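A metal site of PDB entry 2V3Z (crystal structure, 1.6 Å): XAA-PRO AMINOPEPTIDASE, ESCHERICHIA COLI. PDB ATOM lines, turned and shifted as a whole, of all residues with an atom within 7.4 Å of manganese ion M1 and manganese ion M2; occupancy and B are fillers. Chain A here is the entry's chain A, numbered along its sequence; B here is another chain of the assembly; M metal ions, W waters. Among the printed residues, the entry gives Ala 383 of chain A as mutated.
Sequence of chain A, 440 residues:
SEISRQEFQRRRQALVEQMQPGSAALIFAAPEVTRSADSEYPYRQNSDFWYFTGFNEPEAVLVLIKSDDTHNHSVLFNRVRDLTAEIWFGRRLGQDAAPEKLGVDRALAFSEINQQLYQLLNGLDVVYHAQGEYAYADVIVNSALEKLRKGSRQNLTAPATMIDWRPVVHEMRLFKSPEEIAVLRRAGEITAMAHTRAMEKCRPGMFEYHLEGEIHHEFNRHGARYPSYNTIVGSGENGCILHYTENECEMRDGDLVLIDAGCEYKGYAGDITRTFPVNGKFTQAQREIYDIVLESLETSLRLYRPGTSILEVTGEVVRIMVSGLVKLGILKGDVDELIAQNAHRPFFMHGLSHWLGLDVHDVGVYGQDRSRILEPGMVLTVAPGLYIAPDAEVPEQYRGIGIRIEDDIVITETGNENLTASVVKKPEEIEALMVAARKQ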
ATOM      1  N   TYR A 229      11.101   5.250  -2.972  1.00  0.00           N
ATOM      2  CA  TYR A 229      10.854   5.758  -4.314  1.00  0.00           C
ATOM      3  C   TYR A 229      10.391   4.578  -5.142  1.00  0.00           C
ATOM      4  O   TYR A 229      10.569   3.441  -4.755  1.00  0.00           O
ATOM      5  CB  TYR A 229      12.072   6.409  -4.940  1.00  0.00           C
ATOM      6  CG  TYR A 229      13.287   5.545  -4.974  1.00  0.00           C
ATOM      7  CD1 TYR A 229      14.121   5.443  -3.863  1.00  0.00           C
ATOM      8  CD2 TYR A 229      13.627   4.768  -6.091  1.00  0.00           C
ATOM      9  CE1 TYR A 229      15.227   4.623  -3.848  1.00  0.00           C
ATOM     10  CE2 TYR A 229      14.733   3.956  -6.081  1.00  0.00           C
ATOM     11  CZ  TYR A 229      15.518   3.852  -4.955  1.00  0.00           C
ATOM     12  OH  TYR A 229      16.631   3.052  -4.945  1.00  0.00           O
ATOM     13  N   ILE A 232      12.883   0.654  -9.755  1.00  0.00           N
ATOM     14  CA  ILE A 232      13.306   0.555 -11.159  1.00  0.00           C
ATOM     15  C   ILE A 232      13.889  -0.836 -11.416  1.00  0.00           C
ATOM     16  O   ILE A 232      14.827  -1.244 -10.708  1.00  0.00           O
ATOM     17  CB  ILE A 232      14.396   1.629 -11.400  1.00  0.00           C
ATOM     18  CG1 ILE A 232      13.798   3.026 -11.287  1.00  0.00           C
ATOM     19  CG2 ILE A 232      15.146   1.427 -12.720  1.00  0.00           C
ATOM     20  CD1 ILE A 232      14.774   4.124 -10.819  1.00  0.00           C
ATOM     21  N   ILE A 259      18.674  -2.856 -11.243  1.00  0.00           N
ATOM     22  CA  ILE A 259      17.650  -2.687 -10.212  1.00  0.00           C
ATOM     23  C   ILE A 259      18.092  -1.521  -9.350  1.00  0.00           C
ATOM     24  O   ILE A 259      19.148  -1.555  -8.738  1.00  0.00           O
ATOM     25  CB  ILE A 259      17.469  -3.920  -9.354  1.00  0.00           C
ATOM     26  CG1 ILE A 259      17.115  -5.125 -10.242  1.00  0.00           C
ATOM     27  CG2 ILE A 259      16.423  -3.663  -8.276  1.00  0.00           C
ATOM     28  CD1 ILE A 259      16.746  -6.353  -9.437  1.00  0.00           C
ATOM     29  N   ASP A 260      17.262  -0.468  -9.306  1.00  0.00           N
ATOM     30  CA  ASP A 260      17.472   0.687  -8.408  1.00  0.00           C
ATOM     31  C   ASP A 260      16.258   0.696  -7.488  1.00  0.00           C
ATOM     32  O   ASP A 260      15.151   0.917  -7.910  1.00  0.00           O
ATOM     33  CB  ASP A 260      17.591   1.951  -9.272  1.00  0.00           C
ATOM     34  CG  ASP A 260      18.128   3.162  -8.528  1.00  0.00           C
ATOM     35  OD1 ASP A 260      18.087   3.147  -7.286  1.00  0.00           O
ATOM     36  OD2 ASP A 260      18.617   4.090  -9.226  1.00  0.00           O
ATOM     37  N   ALA A 261      16.501   0.362  -6.226  1.00  0.00           N
ATOM     38  CA  ALA A 261      15.430   0.203  -5.274  1.00  0.00           C
ATOM     39  C   ALA A 261      15.930   0.524  -3.877  1.00  0.00           C
ATOM     40  O   ALA A 261      17.073   0.257  -3.530  1.00  0.00           O
ATOM     41  CB  ALA A 261      14.883  -1.227  -5.302  1.00  0.00           C
ATOM     42  N   GLY A 262      15.053   1.093  -3.069  1.00  0.00           N
ATOM     43  CA  GLY A 262      15.396   1.432  -1.703  1.00  0.00           C
ATOM     44  C   GLY A 262      14.187   1.438  -0.806  1.00  0.00           C
ATOM     45  O   GLY A 262      13.076   1.772  -1.255  1.00  0.00           O
ATOM     46  N   GLY A 270      16.804   4.147   2.135  1.00  0.00           N
ATOM     47  CA  GLY A 270      17.884   3.467   1.477  1.00  0.00           C
ATOM     48  C   GLY A 270      17.814   3.715  -0.038  1.00  0.00           C
ATOM     49  O   GLY A 270      16.785   4.100  -0.574  1.00  0.00           O
ATOM     50  N   ASP A 271      18.901   3.462  -0.765  1.00  0.00           N
ATOM     51  CA  ASP A 271      18.956   3.736  -2.216  1.00  0.00           C
ATOM     52  C   ASP A 271      20.130   2.967  -2.769  1.00  0.00           C
ATOM     53  O   ASP A 271      21.260   3.425  -2.713  1.00  0.00           O
ATOM     54  CB  ASP A 271      19.078   5.239  -2.477  1.00  0.00           C
ATOM     55  CG  ASP A 271      19.087   5.584  -3.909  1.00  0.00           C
ATOM     56  OD1 ASP A 271      19.040   4.659  -4.736  1.00  0.00           O
ATOM     57  OD2 ASP A 271      19.165   6.798  -4.223  1.00  0.00           O
ATOM     58  N   ILE A 272      19.889   1.762  -3.309  1.00  0.00           N
ATOM     59  CA  ILE A 272      20.931   0.936  -3.900  1.00  0.00           C
ATOM     60  C   ILE A 272      20.587   0.668  -5.343  1.00  0.00           C
ATOM     61  O   ILE A 272      19.422   0.478  -5.708  1.00  0.00           O
ATOM     62  CB  ILE A 272      21.049  -0.417  -3.177  1.00  0.00           C
ATOM     63  CG1 ILE A 272      21.518  -0.203  -1.745  1.00  0.00           C
ATOM     64  CG2 ILE A 272      21.975  -1.398  -3.929  1.00  0.00           C
ATOM     65  CD1 ILE A 272      21.664  -1.502  -0.934  1.00  0.00           C
ATOM     66  N   THR A 273      21.628   0.641  -6.179  1.00  0.00           N
ATOM     67  CA  THR A 273      21.496   0.083  -7.538  1.00  0.00           C
ATOM     68  C   THR A 273      22.493  -1.057  -7.684  1.00  0.00           C
ATOM     69  O   THR A 273      23.669  -0.908  -7.328  1.00  0.00           O
ATOM     70  CB  THR A 273      21.735   1.077  -8.670  1.00  0.00           C
ATOM     71  OG1 THR A 273      20.925   2.238  -8.487  1.00  0.00           O
ATOM     72  CG2 THR A 273      21.389   0.488 -10.025  1.00  0.00           C
ATOM     73  N   LEU A 352      26.921  12.025  -9.988  1.00  0.00           N
ATOM     74  CA  LEU A 352      27.482  10.899  -9.234  1.00  0.00           C
ATOM     75  C   LEU A 352      26.784  10.654  -7.897  1.00  0.00           C
ATOM     76  O   LEU A 352      26.653   9.505  -7.459  1.00  0.00           O
ATOM     77  CB  LEU A 352      28.961  11.134  -8.981  1.00  0.00           C
ATOM     78  CG  LEU A 352      29.748  10.025  -8.273  1.00  0.00           C
ATOM     79  CD1 LEU A 352      29.840   8.776  -9.148  1.00  0.00           C
ATOM     80  CD2 LEU A 352      31.131  10.555  -7.942  1.00  0.00           C
ATOM     81  N   SER A 353      26.360  11.728  -7.236  1.00  0.00           N
ATOM     82  CA  SER A 353      25.956  11.646  -5.840  1.00  0.00           C
ATOM     83  C   SER A 353      24.871  12.626  -5.497  1.00  0.00           C
ATOM     84  O   SER A 353      24.900  13.759  -5.982  1.00  0.00           O
ATOM     85  CB  SER A 353      27.144  11.979  -4.932  1.00  0.00           C
ATOM     86  OG  SER A 353      28.173  11.011  -5.045  1.00  0.00           O
ATOM     87  N   HIS A 354      23.959  12.200  -4.653  1.00  0.00           N
ATOM     88  CA  HIS A 354      22.977  13.096  -4.060  1.00  0.00           C
ATOM     89  C   HIS A 354      22.903  12.832  -2.573  1.00  0.00           C
ATOM     90  O   HIS A 354      23.187  11.717  -2.093  1.00  0.00           O
ATOM     91  CB  HIS A 354      21.584  12.927  -4.702  1.00  0.00           C
ATOM     92  CG  HIS A 354      21.015  11.551  -4.662  1.00  0.00           C
ATOM     93  ND1 HIS A 354      20.390  11.015  -3.551  1.00  0.00           N
ATOM     94  CD2 HIS A 354      20.930  10.596  -5.633  1.00  0.00           C
ATOM     95  CE1 HIS A 354      19.965   9.785  -3.828  1.00  0.00           C
ATOM     96  NE2 HIS A 354      20.284   9.513  -5.076  1.00  0.00           N
ATOM     97  N   TRP A 355      22.490  13.845  -1.802  1.00  0.00           N
ATOM     98  CA  TRP A 355      22.245  13.652  -0.393  1.00  0.00           C
ATOM     99  C   TRP A 355      21.142  12.612  -0.155  1.00  0.00           C
ATOM    100  O   TRP A 355      20.238  12.490  -0.983  1.00  0.00           O
ATOM    101  CB  TRP A 355      21.796  14.951   0.290  1.00  0.00           C
ATOM    102  CG  TRP A 355      22.616  16.182   0.035  1.00  0.00           C
ATOM    103  CD1 TRP A 355      22.129  17.382  -0.348  1.00  0.00           C
ATOM    104  CD2 TRP A 355      24.032  16.368   0.224  1.00  0.00           C
ATOM    105  NE1 TRP A 355      23.138  18.317  -0.414  1.00  0.00           N
ATOM    106  CE2 TRP A 355      24.316  17.725  -0.063  1.00  0.00           C
ATOM    107  CE3 TRP A 355      25.077  15.539   0.647  1.00  0.00           C
ATOM    108  CZ2 TRP A 355      25.604  18.249  -0.011  1.00  0.00           C
ATOM    109  CZ3 TRP A 355      26.358  16.068   0.705  1.00  0.00           C
ATOM    110  CH2 TRP A 355      26.619  17.416   0.385  1.00  0.00           C
ATOM    111  N   LEU A 356      21.162  11.988   1.012  1.00  0.00           N
ATOM    112  CA  LEU A 356      20.213  10.912   1.367  1.00  0.00           C
ATOM    113  C   LEU A 356      19.706  11.182   2.782  1.00  0.00           C
ATOM    114  O   LEU A 356      20.497  11.552   3.667  1.00  0.00           O
ATOM    115  CB  LEU A 356      20.913   9.559   1.251  1.00  0.00           C
ATOM    116  CG  LEU A 356      20.091   8.292   1.371  1.00  0.00           C
ATOM    117  CD1 LEU A 356      19.175   8.158   0.120  1.00  0.00           C
ATOM    118  CD2 LEU A 356      21.074   7.110   1.501  1.00  0.00           C
ATOM    119  N   VAL A 360      14.774  10.618  -0.496  1.00  0.00           N
ATOM    120  CA  VAL A 360      15.840   9.960  -1.274  1.00  0.00           C
ATOM    121  C   VAL A 360      16.744  10.958  -1.967  1.00  0.00           C
ATOM    122  O   VAL A 360      17.966  10.803  -1.936  1.00  0.00           O
ATOM    123  CB  VAL A 360      15.318   8.856  -2.225  1.00  0.00           C
ATOM    124  CG1 VAL A 360      14.416   9.395  -3.257  1.00  0.00           C
ATOM    125  CG2 VAL A 360      16.503   8.073  -2.821  1.00  0.00           C
ATOM    126  N   HIS A 361      16.160  12.000  -2.552  1.00  0.00           N
ATOM    127  CA  HIS A 361      16.936  13.157  -3.008  1.00  0.00           C
ATOM    128  C   HIS A 361      16.842  14.188  -1.893  1.00  0.00           C
ATOM    129  O   HIS A 361      15.932  15.024  -1.842  1.00  0.00           O
ATOM    130  CB  HIS A 361      16.416  13.711  -4.314  1.00  0.00           C
ATOM    131  CG  HIS A 361      16.634  12.795  -5.468  1.00  0.00           C
ATOM    132  ND1 HIS A 361      15.940  12.936  -6.648  1.00  0.00           N
ATOM    133  CD2 HIS A 361      17.437  11.738  -5.615  1.00  0.00           C
ATOM    134  CE1 HIS A 361      16.338  11.986  -7.490  1.00  0.00           C
ATOM    135  NE2 HIS A 361      17.241  11.234  -6.885  1.00  0.00           N
ATOM    136  N   THR A 381      24.651   9.261  -1.760  1.00  0.00           N
ATOM    137  CA  THR A 381      24.804   8.116  -2.636  1.00  0.00           C
ATOM    138  C   THR A 381      26.059   8.289  -3.488  1.00  0.00           C
ATOM    139  O   THR A 381      26.594   9.397  -3.661  1.00  0.00           O
ATOM    140  CB  THR A 381      23.623   7.964  -3.555  1.00  0.00           C
ATOM    141  OG1 THR A 381      23.512   9.140  -4.394  1.00  0.00           O
ATOM    142  CG2 THR A 381      22.350   7.746  -2.740  1.00  0.00           C
ATOM    143  N   VAL A 382      26.515   7.175  -4.060  1.00  0.00           N
ATOM    144  CA  VAL A 382      27.630   7.171  -4.992  1.00  0.00           C
ATOM    145  C   VAL A 382      27.175   6.232  -6.116  1.00  0.00           C
ATOM    146  O   VAL A 382      27.045   5.037  -5.867  1.00  0.00           O
ATOM    147  CB  VAL A 382      28.899   6.637  -4.352  1.00  0.00           C
ATOM    148  CG1 VAL A 382      30.083   6.800  -5.316  1.00  0.00           C
ATOM    149  CG2 VAL A 382      29.159   7.349  -2.990  1.00  0.00           C
ATOM    150  N   ALA A 383      26.930   6.766  -7.317  1.00  0.00           N
ATOM    151  CA  ALA A 383      26.186   6.043  -8.340  1.00  0.00           C
ATOM    152  C   ALA A 383      26.661   6.307  -9.745  1.00  0.00           C
ATOM    153  O   ALA A 383      25.942   6.855 -10.566  1.00  0.00           O
ATOM    154  CB  ALA A 383      24.706   6.426  -8.232  1.00  0.00           C
ATOM    155  N   ARG A 404      24.441   0.640 -13.824  1.00  0.00           N
ATOM    156  CA  ARG A 404      24.646   1.573 -12.733  1.00  0.00           C
ATOM    157  C   ARG A 404      24.916   0.727 -11.486  1.00  0.00           C
ATOM    158  O   ARG A 404      24.319  -0.342 -11.306  1.00  0.00           O
ATOM    159  CB  ARG A 404      23.408   2.461 -12.504  1.00  0.00           C
ATOM    160  CG  ARG A 404      23.535   3.424 -11.308  1.00  0.00           C
ATOM    161  CD  ARG A 404      22.503   4.543 -11.370  1.00  0.00           C
ATOM    162  NE  ARG A 404      21.087   4.137 -11.267  1.00  0.00           N
ATOM    163  CZ  ARG A 404      20.206   4.140 -12.273  1.00  0.00           C
ATOM    164  NH1 ARG A 404      20.555   4.386 -13.516  1.00  0.00           N
ATOM    165  NH2 ARG A 404      18.910   3.854 -12.030  1.00  0.00           N
ATOM    166  N   GLU A 406      25.379   1.490  -7.308  1.00  0.00           N
ATOM    167  CA  GLU A 406      25.172   2.592  -6.350  1.00  0.00           C
ATOM    168  C   GLU A 406      25.183   2.090  -4.925  1.00  0.00           C
ATOM    169  O   GLU A 406      24.432   1.157  -4.583  1.00  0.00           O
ATOM    170  CB  GLU A 406      23.850   3.249  -6.654  1.00  0.00           C
ATOM    171  CG  GLU A 406      23.366   4.300  -5.668  1.00  0.00           C
ATOM    172  CD  GLU A 406      22.082   4.948  -6.160  1.00  0.00           C
ATOM    173  OE1 GLU A 406      21.215   4.212  -6.725  1.00  0.00           O
ATOM    174  OE2 GLU A 406      21.927   6.167  -5.968  1.00  0.00           O
ATOM    175  N   ASP A 407      25.965   2.788  -4.097  1.00  0.00           N
ATOM    176  CA  ASP A 407      26.024   2.533  -2.652  1.00  0.00           C
ATOM    177  C   ASP A 407      25.649   3.816  -1.916  1.00  0.00           C
ATOM    178  O   ASP A 407      25.679   4.917  -2.473  1.00  0.00           O
ATOM    179  CB  ASP A 407      27.440   2.105  -2.239  1.00  0.00           C
ATOM    180  CG  ASP A 407      27.717   0.597  -2.423  1.00  0.00           C
ATOM    181  OD1 ASP A 407      26.738  -0.220  -2.431  1.00  0.00           O
ATOM    182  OD2 ASP A 407      28.907   0.232  -2.543  1.00  0.00           O
ATOM    183  N   ASP A 408      25.305   3.658  -0.644  1.00  0.00           N
ATOM    184  CA  ASP A 408      25.018   4.795   0.257  1.00  0.00           C
ATOM    185  C   ASP A 408      26.118   4.878   1.291  1.00  0.00           C
ATOM    186  O   ASP A 408      26.492   3.868   1.907  1.00  0.00           O
ATOM    187  CB  ASP A 408      23.718   4.546   1.002  1.00  0.00           C
ATOM    188  CG  ASP A 408      22.560   4.270   0.073  1.00  0.00           C
ATOM    189  OD1 ASP A 408      22.620   4.767  -1.090  1.00  0.00           O
ATOM    190  OD2 ASP A 408      21.615   3.543   0.481  1.00  0.00           O
ATOM    191  N   VAL B   1      18.995   6.492  -7.127  1.00  0.00           N
ATOM    192  CA  VAL B   1      18.034   6.977  -8.170  1.00  0.00           C
ATOM    193  C   VAL B   1      18.583   8.296  -8.631  1.00  0.00           C
ATOM    194  O   VAL B   1      18.677   9.226  -7.835  1.00  0.00           O
ATOM    195  CB  VAL B   1      16.570   7.033  -7.656  1.00  0.00           C
ATOM    196  CG1 VAL B   1      16.468   7.820  -6.367  1.00  0.00           C
ATOM    197  CG2 VAL B   1      15.606   7.621  -8.703  1.00  0.00           C
ATOM    198  N   PRO B   2      19.022   8.367  -9.890  1.00  0.00           N
ATOM    199  CA  PRO B   2      19.797   9.499 -10.348  1.00  0.00           C
ATOM    200  C   PRO B   2      19.107  10.845 -10.187  1.00  0.00           C
ATOM    201  O   PRO B   2      17.900  10.973 -10.435  1.00  0.00           O
ATOM    202  CB  PRO B   2      20.008   9.196 -11.841  1.00  0.00           C
ATOM    203  CG  PRO B   2      19.917   7.719 -11.921  1.00  0.00           C
ATOM    204  CD  PRO B   2      18.894   7.333 -10.935  1.00  0.00           C
ATOM    205  N   LEU B   3      19.905  11.824  -9.780  1.00  0.00           N
ATOM    206  CA  LEU B   3      19.569  13.225  -9.792  1.00  0.00           C
ATOM    207  C   LEU B   3      20.449  13.891 -10.878  1.00  0.00           C
ATOM    208  O   LEU B   3      19.970  14.753 -11.603  1.00  0.00           O
ATOM    209  CB  LEU B   3      19.840  13.829  -8.414  1.00  0.00           C
ATOM    210  CG  LEU B   3      19.465  15.271  -8.148  1.00  0.00           C
ATOM    211  CD1 LEU B   3      17.968  15.516  -8.344  1.00  0.00           C
ATOM    212  CD2 LEU B   3      19.905  15.639  -6.733  1.00  0.00           C
ATOM    213  OXT LEU B   3      21.642  13.570 -11.100  1.00  0.00           O
HETATM  214 MN    MN M   1      19.258   4.769  -6.664  1.00  0.00          MN
HETATM  215 MN    MN M   2      19.946   7.640  -5.923  1.00  0.00          MN
HETATM  216  O   HOH W   1      21.714   7.687  -8.337  1.00  0.00           O
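Manganese ion M2 is bound by N of Val 1 of chain B (1.9 Å), OD2 of Asp 271 (2.1 Å), NE2 of His 354 (2.1 Å) and OE2 of Glu 406 (2.5 Å). Slightly farther from manganese ion M2 lies the backbone carbonyl oxygen (O) of Val 1 of chain B (2.8 Å).
Merely in contact with manganese ion M2: Thr 381 (3.99 Å). Five residues have an atom within 4 Å of manganese ion M2: Asp 271, His 354, Thr 381, Glu 406 and Val 1 of chain B. The nearest printed residue that does not touch manganese ion M2 is Pro 2 of chain B (4.1 Å).
N of Val 1 of chain B binds manganese ion M1 (1.8 Å). OD1 of Asp 271 is bound to manganese ion M1 (1.9 Å). The side-chain carboxylate (OE1) of Glu 406 is bound to manganese ion M1. The side-chain carboxylate (OD1) of Asp 260 binds manganese ion M1, 2.1 Å away. Manganese ion M1 has four donor atoms within binding distance. Slightly farther from manganese ion M1 lies the side-chain carboxylate (OD2) of Asp 260 (2.7 Å).
Residues that only touch manganese ion M1: Tyr 229 (3.6 Å) and Thr 273 (3.5 Å). Six residues have an atom within 4 Å of manganese ion M1: Tyr 229, Asp 260, Asp 271, Thr 273, Glu 406 and Val 1 of chain B. The nearest printed residue that does not touch manganese ion M1 is Ile 272 (4.4 Å).
O of Val 1 of chain B sits at hydrogen-bond distance from NE2 of His 361, at 2.6 Å. OD1 of Asp 271 sits close to OH of Tyr 229, at 2.9 Å. The backbone NH (N) of Asp 271 lies within hydrogen-bond range of the side-chain carboxylate (OD2) of Asp 408 (3.0 Å). The backbone NH (N) of Thr 381 lies within hydrogen-bond range of the backbone carbonyl oxygen (O) of His 354, 2.9 Å away. A ring nitrogen (ND1) of His 354 sits at hydrogen-bond distance from the backbone carbonyl oxygen of Val 360. The side-chain carboxylate of Asp 260 sits close to the side-chain hydroxyl of Thr 273, at 3.1 Å. The backbone NH (N) of Asp 260 lies within hydrogen-bond range of the backbone carbonyl oxygen (O) of Ile 232, at 2.9 Å. The backbone NH of Gly 262 sits at hydrogen-bond distance from the side-chain hydroxyl of Tyr 229, 3.1 Å away.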
